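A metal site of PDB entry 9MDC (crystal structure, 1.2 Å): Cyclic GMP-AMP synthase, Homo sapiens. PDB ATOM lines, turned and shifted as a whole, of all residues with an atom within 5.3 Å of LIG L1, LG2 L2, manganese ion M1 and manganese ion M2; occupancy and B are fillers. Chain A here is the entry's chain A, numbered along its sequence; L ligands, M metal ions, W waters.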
ATOM      1  N   THR A  55      -9.564 -34.836  -1.648  1.00  0.00           N
ATOM      2  CA  THR A  55      -9.539 -33.943  -0.492  1.00  0.00           C
ATOM      3  C   THR A  55     -10.739 -33.017  -0.543  1.00  0.00           C
ATOM      4  O   THR A  55     -11.509 -33.017  -1.508  1.00  0.00           O
ATOM      5  CB  THR A  55      -8.264 -33.073  -0.483  1.00  0.00           C
ATOM      6  OG1 THR A  55      -8.245 -32.226  -1.640  1.00  0.00           O
ATOM      7  CG2 THR A  55      -6.992 -33.927  -0.468  1.00  0.00           C
ATOM      8  N   GLY A  56     -10.870 -32.170   0.497  1.00  0.00           N
ATOM      9  CA  GLY A  56     -11.884 -31.144   0.491  1.00  0.00           C
ATOM     10  C   GLY A  56     -13.278 -31.653   0.798  1.00  0.00           C
ATOM     11  O   GLY A  56     -13.515 -32.834   1.116  1.00  0.00           O
ATOM     12  N   SER A  57     -14.245 -30.735   0.670  1.00  0.00           N
ATOM     13  CA  SER A  57     -15.531 -30.941   1.337  1.00  0.00           C
ATOM     14  C   SER A  57     -16.332 -32.101   0.764  1.00  0.00           C
ATOM     15  O   SER A  57     -17.099 -32.724   1.494  1.00  0.00           O
ATOM     16  CB  SER A  57     -16.376 -29.673   1.307  1.00  0.00           C
ATOM     17  OG  SER A  57     -16.721 -29.332  -0.027  1.00  0.00           O
ATOM     18  N   TYR A  58     -16.216 -32.390  -0.542  1.00  0.00           N
ATOM     19  CA  TYR A  58     -17.005 -33.490  -1.094  1.00  0.00           C
ATOM     20  C   TYR A  58     -16.604 -34.789  -0.424  1.00  0.00           C
ATOM     21  O   TYR A  58     -17.464 -35.594  -0.032  1.00  0.00           O
ATOM     22  CB  TYR A  58     -16.807 -33.564  -2.606  1.00  0.00           C
ATOM     23  CG  TYR A  58     -17.561 -34.686  -3.257  1.00  0.00           C
ATOM     24  CD1 TYR A  58     -18.872 -34.511  -3.699  1.00  0.00           C
ATOM     25  CD2 TYR A  58     -16.973 -35.929  -3.440  1.00  0.00           C
ATOM     26  CE1 TYR A  58     -19.569 -35.546  -4.309  1.00  0.00           C
ATOM     27  CE2 TYR A  58     -17.656 -36.968  -4.051  1.00  0.00           C
ATOM     28  CZ  TYR A  58     -18.951 -36.766  -4.485  1.00  0.00           C
ATOM     29  OH  TYR A  58     -19.633 -37.774  -5.103  1.00  0.00           O
ATOM     30  N   GLU A  60     -15.088 -35.103   2.452  1.00  0.00           N
ATOM     31  CA  GLU A  60     -15.347 -34.980   3.881  1.00  0.00           C
ATOM     32  C   GLU A  60     -16.834 -34.990   4.200  1.00  0.00           C
ATOM     33  O   GLU A  60     -17.209 -34.863   5.370  1.00  0.00           O
ATOM     34  CB  GLU A  60     -14.698 -33.680   4.402  1.00  0.00           C
ATOM     35  CG  GLU A  60     -13.174 -33.691   4.330  1.00  0.00           C
ATOM     36  CD  GLU A  60     -12.536 -32.316   4.391  1.00  0.00           C
ATOM     37  OE1 GLU A  60     -11.334 -32.228   4.716  1.00  0.00           O
ATOM     38  OE2 GLU A  60     -13.259 -31.315   4.173  1.00  0.00           O
ATOM     39  N   VAL A  62     -19.074 -32.771   3.699  1.00  0.00           N
ATOM     40  CA  VAL A  62     -19.588 -31.476   4.156  1.00  0.00           C
ATOM     41  C   VAL A  62     -19.771 -30.515   2.976  1.00  0.00           C
ATOM     42  O   VAL A  62     -19.924 -29.299   3.177  1.00  0.00           O
ATOM     43  CB  VAL A  62     -18.761 -30.866   5.306  1.00  0.00           C
ATOM     44  CG1 VAL A  62     -18.832 -31.749   6.576  1.00  0.00           C
ATOM     45  CG2 VAL A  62     -17.311 -30.625   4.876  1.00  0.00           C
ATOM     46  N   LYS A  63     -19.790 -31.035   1.751  1.00  0.00           N
ATOM     47  CA  LYS A  63     -20.179 -30.221   0.604  1.00  0.00           C
ATOM     48  C   LYS A  63     -21.664 -29.909   0.698  1.00  0.00           C
ATOM     49  O   LYS A  63     -22.470 -30.793   0.996  1.00  0.00           O
ATOM     50  CB  LYS A  63     -19.871 -30.975  -0.687  1.00  0.00           C
ATOM     51  CG  LYS A  63     -20.234 -30.232  -1.955  1.00  0.00           C
ATOM     52  CD  LYS A  63     -19.165 -29.207  -2.302  1.00  0.00           C
ATOM     53  CE  LYS A  63     -19.563 -28.297  -3.469  1.00  0.00           C
ATOM     54  NZ  LYS A  63     -20.674 -27.355  -3.098  1.00  0.00           N
ATOM     55  N   ILE A  64     -22.036 -28.648   0.451  1.00  0.00           N
ATOM     56  CA  ILE A  64     -23.428 -28.228   0.586  1.00  0.00           C
ATOM     57  C   ILE A  64     -24.017 -27.814  -0.756  1.00  0.00           C
ATOM     58  O   ILE A  64     -23.299 -27.459  -1.691  1.00  0.00           O
ATOM     59  CB  ILE A  64     -23.638 -27.128   1.650  1.00  0.00           C
ATOM     60  CG1 ILE A  64     -22.848 -25.853   1.311  1.00  0.00           C
ATOM     61  CG2 ILE A  64     -23.265 -27.676   3.039  1.00  0.00           C
ATOM     62  CD1 ILE A  64     -23.138 -24.687   2.258  1.00  0.00           C
ATOM     63  N   GLU A  69     -18.205 -28.841  -6.900  1.00  0.00           N
ATOM     64  CA  GLU A  69     -16.828 -28.409  -6.676  1.00  0.00           C
ATOM     65  C   GLU A  69     -16.080 -29.520  -5.950  1.00  0.00           C
ATOM     66  O   GLU A  69     -16.478 -29.930  -4.846  1.00  0.00           O
ATOM     67  CB  GLU A  69     -16.739 -27.076  -5.930  1.00  0.00           C
ATOM     68  CG  GLU A  69     -15.415 -26.316  -6.163  1.00  0.00           C
ATOM     69  CD  GLU A  69     -14.345 -26.626  -5.158  1.00  0.00           C
ATOM     70  OE1 GLU A  69     -14.579 -27.409  -4.215  1.00  0.00           O
ATOM     71  OE2 GLU A  69     -13.259 -26.024  -5.302  1.00  0.00           O
ATOM     72  N   PHE A  70     -15.028 -30.017  -6.593  1.00  0.00           N
ATOM     73  CA  PHE A  70     -14.249 -31.149  -6.122  1.00  0.00           C
ATOM     74  C   PHE A  70     -12.791 -30.731  -6.028  1.00  0.00           C
ATOM     75  O   PHE A  70     -12.296 -29.953  -6.843  1.00  0.00           O
ATOM     76  CB  PHE A  70     -14.301 -32.316  -7.117  1.00  0.00           C
ATOM     77  CG  PHE A  70     -15.650 -32.985  -7.221  1.00  0.00           C
ATOM     78  CD1 PHE A  70     -16.697 -32.379  -7.901  1.00  0.00           C
ATOM     79  CD2 PHE A  70     -15.872 -34.233  -6.649  1.00  0.00           C
ATOM     80  CE1 PHE A  70     -17.935 -32.998  -8.001  1.00  0.00           C
ATOM     81  CE2 PHE A  70     -17.100 -34.866  -6.778  1.00  0.00           C
ATOM     82  CZ  PHE A  70     -18.133 -34.242  -7.450  1.00  0.00           C
ATOM     83  N   ASP A  71     -12.075 -31.331  -5.072  1.00  0.00           N
ATOM     84  CA  ASP A  71     -10.658 -31.058  -4.865  1.00  0.00           C
ATOM     85  C   ASP A  71      -9.882 -32.357  -4.861  1.00  0.00           C
ATOM     86  O   ASP A  71     -10.234 -33.314  -4.171  1.00  0.00           O
ATOM     87  CB  ASP A  71     -10.443 -30.336  -3.544  1.00  0.00           C
ATOM     88  CG  ASP A  71     -11.290 -29.109  -3.440  1.00  0.00           C
ATOM     89  OD1 ASP A  71     -10.898 -28.101  -4.067  1.00  0.00           O
ATOM     90  OD2 ASP A  71     -12.326 -29.150  -2.743  1.00  0.00           O
ATOM     91  N   GLY A 148      -2.390 -16.926  -6.208  1.00  0.00           N
ATOM     92  CA  GLY A 148      -2.370 -17.534  -4.889  1.00  0.00           C
ATOM     93  C   GLY A 148      -2.977 -18.918  -4.796  1.00  0.00           C
ATOM     94  O   GLY A 148      -3.048 -19.468  -3.686  1.00  0.00           O
ATOM     95  N   SER A 149      -3.424 -19.496  -5.913  1.00  0.00           N
ATOM     96  CA  SER A 149      -3.876 -20.884  -5.774  1.00  0.00           C
ATOM     97  C   SER A 149      -2.799 -21.827  -6.285  1.00  0.00           C
ATOM     98  O   SER A 149      -2.175 -21.558  -7.310  1.00  0.00           O
ATOM     99  CB  SER A 149      -5.147 -21.109  -6.593  1.00  0.00           C
ATOM    100  OG  SER A 149      -5.509 -22.483  -6.583  1.00  0.00           O
ATOM    101  N   PRO A 150      -2.559 -22.931  -5.568  1.00  0.00           N
ATOM    102  CA  PRO A 150      -1.632 -23.953  -6.083  1.00  0.00           C
ATOM    103  C   PRO A 150      -2.286 -24.887  -7.083  1.00  0.00           C
ATOM    104  O   PRO A 150      -1.600 -25.774  -7.606  1.00  0.00           O
ATOM    105  CB  PRO A 150      -1.242 -24.705  -4.801  1.00  0.00           C
ATOM    106  CG  PRO A 150      -2.487 -24.641  -3.965  1.00  0.00           C
ATOM    107  CD  PRO A 150      -3.079 -23.272  -4.234  1.00  0.00           C
ATOM    108  N   ALA A 151      -3.576 -24.729  -7.362  1.00  0.00           N
ATOM    109  CA  ALA A 151      -4.325 -25.675  -8.169  1.00  0.00           C
ATOM    110  C   ALA A 151      -4.451 -25.233  -9.621  1.00  0.00           C
ATOM    111  O   ALA A 151      -4.411 -24.045  -9.956  1.00  0.00           O
ATOM    112  CB  ALA A 151      -5.727 -25.867  -7.598  1.00  0.00           C
ATOM    113  N   ASP A 163     -10.547 -28.720  -8.726  1.00  0.00           N
ATOM    114  CA  ASP A 163      -9.209 -28.204  -8.423  1.00  0.00           C
ATOM    115  C   ASP A 163      -8.228 -29.366  -8.353  1.00  0.00           C
ATOM    116  O   ASP A 163      -8.393 -30.254  -7.526  1.00  0.00           O
ATOM    117  CB  ASP A 163      -9.229 -27.452  -7.089  1.00  0.00           C
ATOM    118  CG  ASP A 163      -9.996 -26.146  -7.142  1.00  0.00           C
ATOM    119  OD1 ASP A 163     -10.149 -25.601  -8.261  1.00  0.00           O
ATOM    120  OD2 ASP A 163     -10.433 -25.677  -6.083  1.00  0.00           O
ATOM    121  N   THR A 165      -4.423 -30.145  -7.544  1.00  0.00           N
ATOM    122  CA  THR A 165      -3.219 -29.587  -6.920  1.00  0.00           C
ATOM    123  C   THR A 165      -2.070 -30.571  -7.009  1.00  0.00           C
ATOM    124  O   THR A 165      -2.128 -31.669  -6.439  1.00  0.00           O
ATOM    125  CB  THR A 165      -3.486 -29.200  -5.461  1.00  0.00           C
ATOM    126  OG1 THR A 165      -4.526 -28.218  -5.410  1.00  0.00           O
ATOM    127  CG2 THR A 165      -2.234 -28.604  -4.845  1.00  0.00           C
ATOM    128  N   VAL A 204       2.816 -28.123  -1.662  1.00  0.00           N
ATOM    129  CA  VAL A 204       2.064 -27.701  -2.837  1.00  0.00           C
ATOM    130  C   VAL A 204       2.657 -26.398  -3.376  1.00  0.00           C
ATOM    131  O   VAL A 204       3.263 -25.629  -2.609  1.00  0.00           O
ATOM    132  CB  VAL A 204       0.557 -27.580  -2.531  1.00  0.00           C
ATOM    133  CG1 VAL A 204       0.031 -28.904  -1.994  1.00  0.00           C
ATOM    134  CG2 VAL A 204       0.273 -26.448  -1.543  1.00  0.00           C
ATOM    135  N   LYS A 206       2.184 -23.301  -3.810  1.00  0.00           N
ATOM    136  CA  LYS A 206       1.704 -21.986  -3.424  1.00  0.00           C
ATOM    137  C   LYS A 206       2.886 -21.223  -2.862  1.00  0.00           C
ATOM    138  O   LYS A 206       3.549 -21.702  -1.933  1.00  0.00           O
ATOM    139  CB  LYS A 206       0.595 -22.077  -2.379  1.00  0.00           C
ATOM    140  CG  LYS A 206       0.141 -20.706  -1.916  1.00  0.00           C
ATOM    141  CD  LYS A 206      -1.106 -20.746  -1.080  1.00  0.00           C
ATOM    142  CE  LYS A 206      -1.407 -19.369  -0.507  1.00  0.00           C
ATOM    143  NZ  LYS A 206      -1.389 -18.312  -1.557  1.00  0.00           N
ATOM    144  N   ARG A 220       4.448 -24.747  -0.186  1.00  0.00           N
ATOM    145  CA  ARG A 220       3.737 -24.592   1.070  1.00  0.00           C
ATOM    146  C   ARG A 220       3.297 -25.951   1.611  1.00  0.00           C
ATOM    147  O   ARG A 220       2.863 -26.836   0.854  1.00  0.00           O
ATOM    148  CB  ARG A 220       2.509 -23.700   0.905  1.00  0.00           C
ATOM    149  CG  ARG A 220       1.784 -23.447   2.204  1.00  0.00           C
ATOM    150  CD  ARG A 220       0.911 -22.244   2.125  1.00  0.00           C
ATOM    151  NE  ARG A 220      -0.011 -22.162   3.251  1.00  0.00           N
ATOM    152  CZ  ARG A 220      -0.818 -21.134   3.474  1.00  0.00           C
ATOM    153  NH1 ARG A 220      -0.751 -20.039   2.734  1.00  0.00           N
ATOM    154  NH2 ARG A 220      -1.729 -21.223   4.436  1.00  0.00           N
ATOM    155  N   LEU A 221       3.400 -26.136   2.931  1.00  0.00           N
ATOM    156  CA  LEU A 221       2.949 -27.366   3.551  1.00  0.00           C
ATOM    157  C   LEU A 221       1.445 -27.540   3.403  1.00  0.00           C
ATOM    158  O   LEU A 221       0.675 -26.577   3.525  1.00  0.00           O
ATOM    159  CB  LEU A 221       3.293 -27.383   5.042  1.00  0.00           C
ATOM    160  CG  LEU A 221       4.773 -27.431   5.438  1.00  0.00           C
ATOM    161  CD1 LEU A 221       4.918 -27.324   6.948  1.00  0.00           C
ATOM    162  CD2 LEU A 221       5.422 -28.714   4.907  1.00  0.00           C
ATOM    163  N   SER A 222       1.007 -28.777   3.167  1.00  0.00           N
ATOM    164  CA  SER A 222      -0.410 -29.091   3.165  1.00  0.00           C
ATOM    165  C   SER A 222      -0.659 -30.351   3.964  1.00  0.00           C
ATOM    166  O   SER A 222       0.036 -31.365   3.787  1.00  0.00           O
ATOM    167  CB  SER A 222      -0.937 -29.271   1.741  1.00  0.00           C
ATOM    168  OG  SER A 222      -2.312 -29.597   1.780  1.00  0.00           O
ATOM    169  N   SER A 224      -4.020 -31.510   4.054  1.00  0.00           N
ATOM    170  CA  SER A 224      -5.423 -31.673   3.691  1.00  0.00           C
ATOM    171  C   SER A 224      -5.902 -33.106   3.887  1.00  0.00           C
ATOM    172  O   SER A 224      -7.089 -33.342   4.170  1.00  0.00           O
ATOM    173  CB  SER A 224      -5.633 -31.217   2.242  1.00  0.00           C
ATOM    174  OG  SER A 224      -7.004 -31.202   1.900  1.00  0.00           O
ATOM    175  N   GLU A 227      -6.827 -33.402   7.586  1.00  0.00           N
ATOM    176  CA  GLU A 227      -8.126 -32.780   7.805  1.00  0.00           C
ATOM    177  C   GLU A 227      -9.253 -33.716   7.424  1.00  0.00           C
ATOM    178  O   GLU A 227     -10.262 -33.817   8.149  1.00  0.00           O
ATOM    179  CB  GLU A 227      -8.213 -31.482   7.007  1.00  0.00           C
ATOM    180  CG  GLU A 227      -7.151 -30.495   7.424  1.00  0.00           C
ATOM    181  CD  GLU A 227      -7.057 -29.272   6.522  1.00  0.00           C
ATOM    182  OE1 GLU A 227      -7.888 -29.108   5.595  1.00  0.00           O
ATOM    183  OE2 GLU A 227      -6.142 -28.461   6.744  1.00  0.00           O
ATOM    184  N   LYS A 258     -20.297 -22.680   7.036  1.00  0.00           N
ATOM    185  CA  LYS A 258     -19.901 -22.448   5.648  1.00  0.00           C
ATOM    186  C   LYS A 258     -20.989 -21.704   4.879  1.00  0.00           C
ATOM    187  O   LYS A 258     -20.696 -20.812   4.084  1.00  0.00           O
ATOM    188  CB  LYS A 258     -19.568 -23.761   4.962  1.00  0.00           C
ATOM    189  CG  LYS A 258     -19.159 -23.554   3.510  1.00  0.00           C
ATOM    190  CD  LYS A 258     -18.378 -24.741   2.991  1.00  0.00           C
ATOM    191  CE  LYS A 258     -19.140 -26.036   3.180  1.00  0.00           C
ATOM    192  NZ  LYS A 258     -18.318 -27.194   2.730  1.00  0.00           N
ATOM    193  N   SER A 279     -13.853 -20.559   2.943  1.00  0.00           N
ATOM    194  CA  SER A 279     -14.352 -21.650   3.771  1.00  0.00           C
ATOM    195  C   SER A 279     -13.245 -22.242   4.639  1.00  0.00           C
ATOM    196  O   SER A 279     -13.554 -22.815   5.691  1.00  0.00           O
ATOM    197  CB  SER A 279     -15.081 -22.696   2.942  1.00  0.00           C
ATOM    198  OG  SER A 279     -14.146 -23.377   2.173  1.00  0.00           O
ATOM    199  N   TYR A 280     -11.964 -22.076   4.270  1.00  0.00           N
ATOM    200  CA  TYR A 280     -10.897 -22.604   5.126  1.00  0.00           C
ATOM    201  C   TYR A 280     -10.817 -21.862   6.443  1.00  0.00           C
ATOM    202  O   TYR A 280     -10.401 -22.434   7.463  1.00  0.00           O
ATOM    203  CB  TYR A 280      -9.541 -22.555   4.414  1.00  0.00           C
ATOM    204  CG  TYR A 280      -8.522 -23.424   5.114  1.00  0.00           C
ATOM    205  CD1 TYR A 280      -8.643 -24.808   5.110  1.00  0.00           C
ATOM    206  CD2 TYR A 280      -7.439 -22.882   5.797  1.00  0.00           C
ATOM    207  CE1 TYR A 280      -7.735 -25.623   5.749  1.00  0.00           C
ATOM    208  CE2 TYR A 280      -6.521 -23.690   6.443  1.00  0.00           C
ATOM    209  CZ  TYR A 280      -6.668 -25.056   6.412  1.00  0.00           C
ATOM    210  OH  TYR A 280      -5.755 -25.830   7.058  1.00  0.00           O
ATOM    211  N   LYS A 283     -13.414 -23.612   8.414  1.00  0.00           N
ATOM    212  CA  LYS A 283     -12.942 -24.965   8.708  1.00  0.00           C
ATOM    213  C   LYS A 283     -11.928 -24.955   9.836  1.00  0.00           C
ATOM    214  O   LYS A 283     -11.987 -25.770  10.767  1.00  0.00           O
ATOM    215  CB  LYS A 283     -12.347 -25.576   7.431  1.00  0.00           C
ATOM    216  CG  LYS A 283     -12.111 -27.078   7.496  1.00  0.00           C
ATOM    217  CD  LYS A 283     -11.335 -27.587   6.273  1.00  0.00           C
ATOM    218  CE  LYS A 283     -11.443 -29.111   6.141  1.00  0.00           C
ATOM    219  NZ  LYS A 283     -10.590 -29.642   5.036  1.00  0.00           N
ATOM    220  N   ASN A 326      -3.425 -21.412  12.250  1.00  0.00           N
ATOM    221  CA  ASN A 326      -3.503 -22.633  11.468  1.00  0.00           C
ATOM    222  C   ASN A 326      -3.494 -23.835  12.403  1.00  0.00           C
ATOM    223  O   ASN A 326      -2.788 -23.857  13.411  1.00  0.00           O
ATOM    224  CB  ASN A 326      -2.326 -22.667  10.491  1.00  0.00           C
ATOM    225  CG  ASN A 326      -2.330 -23.900   9.601  1.00  0.00           C
ATOM    226  OD1 ASN A 326      -1.916 -24.964  10.025  1.00  0.00           O
ATOM    227  ND2 ASN A 326      -2.791 -23.733   8.361  1.00  0.00           N
HETATM  228  C1  LIG L   1      -3.475 -26.160  -0.149  1.00  0.00           C
HETATM  229  C2  LIG L   1      -7.584 -22.299  -3.554  1.00  0.00           C
HETATM  230  C3  LIG L   1      -7.040 -24.644  -2.878  1.00  0.00           C
HETATM  231  C4  LIG L   1      -9.328 -24.081  -3.365  1.00  0.00           C
HETATM  232  C5  LIG L   1     -10.518 -23.159  -3.544  1.00  0.00           C
HETATM  233  C6  LIG L   1     -12.685 -22.936  -4.240  1.00  0.00           C
HETATM  234  C7  LIG L   1     -12.697 -21.615  -3.845  1.00  0.00           C
HETATM  235  C8  LIG L   1     -11.541 -21.137  -3.255  1.00  0.00           C
HETATM  236  C9  LIG L   1     -15.101 -21.403  -4.118  1.00  0.00           C
HETATM  237  C10 LIG L   1     -16.102 -20.287  -4.152  1.00  0.00           C
HETATM  238  C11 LIG L   1      -6.475 -25.308  -4.126  1.00  0.00           C
HETATM  239  C12 LIG L   1      -2.844 -25.127   0.526  1.00  0.00           C
HETATM  240  C13 LIG L   1      -3.244 -23.816   0.309  1.00  0.00           C
HETATM  241  C14 LIG L   1      -4.302 -23.552  -0.549  1.00  0.00           C
HETATM  242  C15 LIG L   1      -4.963 -24.608  -1.217  1.00  0.00           C
HETATM  243  C16 LIG L   1      -4.535 -25.927  -1.014  1.00  0.00           C
HETATM  244  C17 LIG L   1      -5.936 -22.666  -1.785  1.00  0.00           C
HETATM  245  C18 LIG L   1      -5.998 -24.005  -2.009  1.00  0.00           C
HETATM  246  C19 LIG L   1      -6.863 -21.646  -2.373  1.00  0.00           C
HETATM  247  N1  LIG L   1      -4.910 -22.377  -0.917  1.00  0.00           N
HETATM  248  N2  LIG L   1      -8.054 -23.639  -3.238  1.00  0.00           N
HETATM  249  N3  LIG L   1     -11.604 -23.700  -4.093  1.00  0.00           N
HETATM  250  N4  LIG L   1     -10.459 -21.901  -3.094  1.00  0.00           N
HETATM  251  O1  LIG L   1      -9.609 -25.281  -3.357  1.00  0.00           O
HETATM  252  O2  LIG L   1     -13.803 -20.812  -3.984  1.00  0.00           O
HETATM  253  O3  LIG L   1     -15.780 -19.352  -5.167  1.00  0.00           O
HETATM  254 CL1  LIG L   1      -1.542 -25.485   1.632  1.00  0.00          CL
HETATM  255 CL2  LIG L   1      -2.497 -22.483   1.117  1.00  0.00          CL
HETATM  256  P1  LG2 L   2     -16.036 -25.967  -0.184  1.00  0.00           P
HETATM  257  O1  LG2 L   2     -16.244 -24.463  -0.030  1.00  0.00           O
HETATM  258  O2  LG2 L   2     -15.350 -26.376  -1.461  1.00  0.00           O
HETATM  259  O3  LG2 L   2     -17.286 -26.760   0.140  1.00  0.00           O
HETATM  260  P2  LG2 L   2     -13.463 -27.033   0.895  1.00  0.00           P
HETATM  261  O4  LG2 L   2     -12.890 -27.327   2.230  1.00  0.00           O
HETATM  262  O5  LG2 L   2     -13.448 -28.095  -0.165  1.00  0.00           O
HETATM  263  N1  LG2 L   2     -14.956 -26.415   1.118  1.00  0.00           N
HETATM  264  P3  LG2 L   2     -11.716 -25.444  -0.937  1.00  0.00           P
HETATM  265  O6  LG2 L   2     -11.553 -23.968  -0.976  1.00  0.00           O
HETATM  266  O7  LG2 L   2     -12.263 -26.149  -2.165  1.00  0.00           O
HETATM  267  O8  LG2 L   2     -12.593 -25.740   0.335  1.00  0.00           O
HETATM  268  O9  LG2 L   2     -10.295 -26.059  -0.536  1.00  0.00           O
HETATM  269  C1  LG2 L   2     -10.053 -27.448  -0.661  1.00  0.00           C
HETATM  270  C2  LG2 L   2      -9.085 -27.883   0.424  1.00  0.00           C
HETATM  271  O10 LG2 L   2      -7.816 -27.211   0.234  1.00  0.00           O
HETATM  272  C3  LG2 L   2      -9.452 -27.508   1.863  1.00  0.00           C
HETATM  273  O11 LG2 L   2     -10.410 -28.356   2.427  1.00  0.00           O
HETATM  274  C4  LG2 L   2      -8.098 -27.486   2.538  1.00  0.00           C
HETATM  275  O12 LG2 L   2      -7.756 -28.810   2.913  1.00  0.00           O
HETATM  276  C5  LG2 L   2      -7.170 -26.933   1.422  1.00  0.00           C
HETATM  277  N2  LG2 L   2      -7.021 -25.495   1.559  1.00  0.00           N
HETATM  278  C6  LG2 L   2      -7.779 -24.484   1.017  1.00  0.00           C
HETATM  279  N3  LG2 L   2      -7.402 -23.291   1.388  1.00  0.00           N
HETATM  280  C7  LG2 L   2      -6.340 -23.515   2.224  1.00  0.00           C
HETATM  281  C8  LG2 L   2      -5.488 -22.663   2.957  1.00  0.00           C
HETATM  282  N4  LG2 L   2      -5.609 -21.321   2.945  1.00  0.00           N
HETATM  283  N5  LG2 L   2      -4.543 -23.217   3.710  1.00  0.00           N
HETATM  284  C9  LG2 L   2      -4.416 -24.540   3.736  1.00  0.00           C
HETATM  285  N6  LG2 L   2      -5.144 -25.430   3.099  1.00  0.00           N
HETATM  286  C10 LG2 L   2      -6.096 -24.873   2.353  1.00  0.00           C
HETATM  287 MN    MN M   1     -11.434 -26.039  -4.243  1.00  0.00          MN
HETATM  288 MN    MN M   2     -13.868 -27.692  -2.232  1.00  0.00          MN
HETATM  289  O   HOH W   1      -9.532 -19.492  -1.287  1.00  0.00           O
HETATM  290  O   HOH W   2     -15.836 -24.396  -3.378  1.00  0.00           O
HETATM  291  O   HOH W   3      -7.841 -18.977   3.010  1.00  0.00           O
HETATM  292  O   HOH W   4      -3.665 -21.846   6.255  1.00  0.00           O
HETATM  293  O   HOH W   5     -11.263 -22.545   1.379  1.00  0.00           O
HETATM  294  O   HOH W   6     -19.979 -26.555  -0.381  1.00  0.00           O
HETATM  295  O   HOH W   7     -14.247 -22.801  -1.061  1.00  0.00           O
HETATM  296  O   HOH W   8      -4.879 -19.481  -0.049  1.00  0.00           O
HETATM  297  O   HOH W   9      -4.145 -28.028   3.197  1.00  0.00           O
HETATM  298  O   HOH W  10     -11.612 -24.994   3.300  1.00  0.00           O
HETATM  299  O   HOH W  11     -15.254 -29.467  -2.299  1.00  0.00           O
HETATM  300  O   HOH W  12     -14.299 -28.799   4.047  1.00  0.00           O
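Ser 149 touches LIG L1.
Pro 150 touches LIG L1.
Ala 151 touches LIG L1 (CB to C11, 3.6 Å).
Thr 165 touches LIG L1.
Val 204 touches LIG L1.
Lys 206 touches LIG L1.
Arg 220 touches LIG L1.
Leu 221 touches LIG L1 (O to CL1, 3.1 Å).
CB of Ser 222 touches CL1 of LIG L1, at 3.8 Å.
Hydrophobic or aromatic side chains that line LIG L1: Pro 150, Ala 151 and Val 204.
Of the 29 residues printed, 12 come within 4 Å of LIG L1.
Manganese ion M2 is bound by the side-chain carboxylate (OE1) of Glu 69 (2.1 Å), an oxygen (O2) of LG2 L2 (2.1 Å), an oxygen (O5) of LG2 L2 (2.1 Å), the side-chain carboxylate (OD2) of Asp 71 (2.2 Å), an oxygen (O7) of LG2 L2 (2.2 Å) and water W11 (2.3 Å).
Manganese ion M2 has six donor atoms within binding distance.
Manganese ion M1 is bound by OE2 of Glu 69 (2.1 Å).
OD2 of Asp 163 binds manganese ion M1 (2.1 Å).
The side-chain carboxylate (OD1) of Asp 71 binds manganese ion M1 (2.1 Å).
Manganese ion M1 is bound by O1 of LIG L1, 2.2 Å away.
O7 of LG2 L2 binds manganese ion M1, 2.2 Å away.
N3 of LIG L1 is bound to manganese ion M1, 2.3 Å away.
N of Val 62 lies within hydrogen-bond range of O of Ser 57 (3.0 Å).
NZ of Lys 258 lies within hydrogen-bond range of O of Val 62, 2.7 Å away.
O of Arg 220 sits at hydrogen-bond distance from N of Val 204.
The backbone carbonyl oxygen of Phe 70 sits at hydrogen-bond distance from the backbone NH of Asp 163 (2.9 Å).
NZ of Lys 206 sits at hydrogen-bond distance from O of Gly 148 (2.9 Å).
The side-chain hydroxyl of Ser 149 is in hydrogen-bond range of the backbone NH of Ala 151.
NZ of Lys 283 is in salt-bridge range of OE1 of Glu 60 (2.7 Å).
The backbone carbonyl oxygen (O) of Ser 57 is in hydrogen-bond range of the backbone NH (N) of Lys 63, at 3.2 Å.
CA of Gly 56 touches O5 of LG2 L2 (3.5 Å).
Lys 63 touches LG2 L2 (CD to O3, 3.9 Å).
NH2 of Arg 220 touches N5 of LG2 L2 (3.5 Å).
Tyr 280 touches LG2 L2 (CE2 to N5, 3.4 Å).
Hydrophobic or aromatic side chains that line LG2 L2: Tyr 280.
12 residues have an atom within 4 Å of LG2 L2: Gly 56, Ser 57, Lys 63, Glu 69, Asp 71, Arg 220, Ser 224, Glu 227, Lys 258, Ser 279, Tyr 280 and Lys 283.
Merely in contact with manganese ion M2: Ser 57 (3.96 Å).
Of the 29 residues printed, 3 come within 4 Å of manganese ion M2.
Water W11 bridges OG of Ser 57 (2.7 Å) and O of Glu 69 (2.9 Å).
Water W6 lies within hydrogen-bond range of O3 of LG2 L2, NZ of Lys 63 and N of Ile 64.
Water W9 lies within hydrogen-bond range of N6 of LG2 L2 (2.8 Å) and OG of Ser 222 (2.8 Å).
Water W7 lies within hydrogen-bond range of O1 of LG2 L2 (2.8 Å) and OG of Ser 279 (3.3 Å).
Water W10 lies within hydrogen-bond range of an oxygen (O4) of LG2 L2, the backbone NH of Tyr 280 and the side-chain hydroxyl of Ser 279.
Water W4 lies within hydrogen-bond range of NH2 of Arg 220, ND2 of Asn 326 and N5 of LG2 L2.
The side-chain carboxylate (OE1) of Glu 227 lies within hydrogen-bond range of an oxygen (O12) of LG2 L2 (2.7 Å).
NZ of Lys 283 lies within hydrogen-bond range of O11 of LG2 L2 (2.9 Å).
N of Ser 57 sits close to O5 of LG2 L2, at 2.9 Å.
OG of Ser 279 lies within hydrogen-bond range of O1 of LG2 L2 (3.2 Å).
An oxygen (O3) of LG2 L2 sits at hydrogen-bond distance from the side-chain hydroxyl of Ser 57 (2.6 Å).
O3 of LG2 L2 is in salt-bridge range of NZ of Lys 258.
The side-chain hydroxyl of Ser 224 lies within hydrogen-bond range of an oxygen (O12) of LG2 L2, 2.7 Å away.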
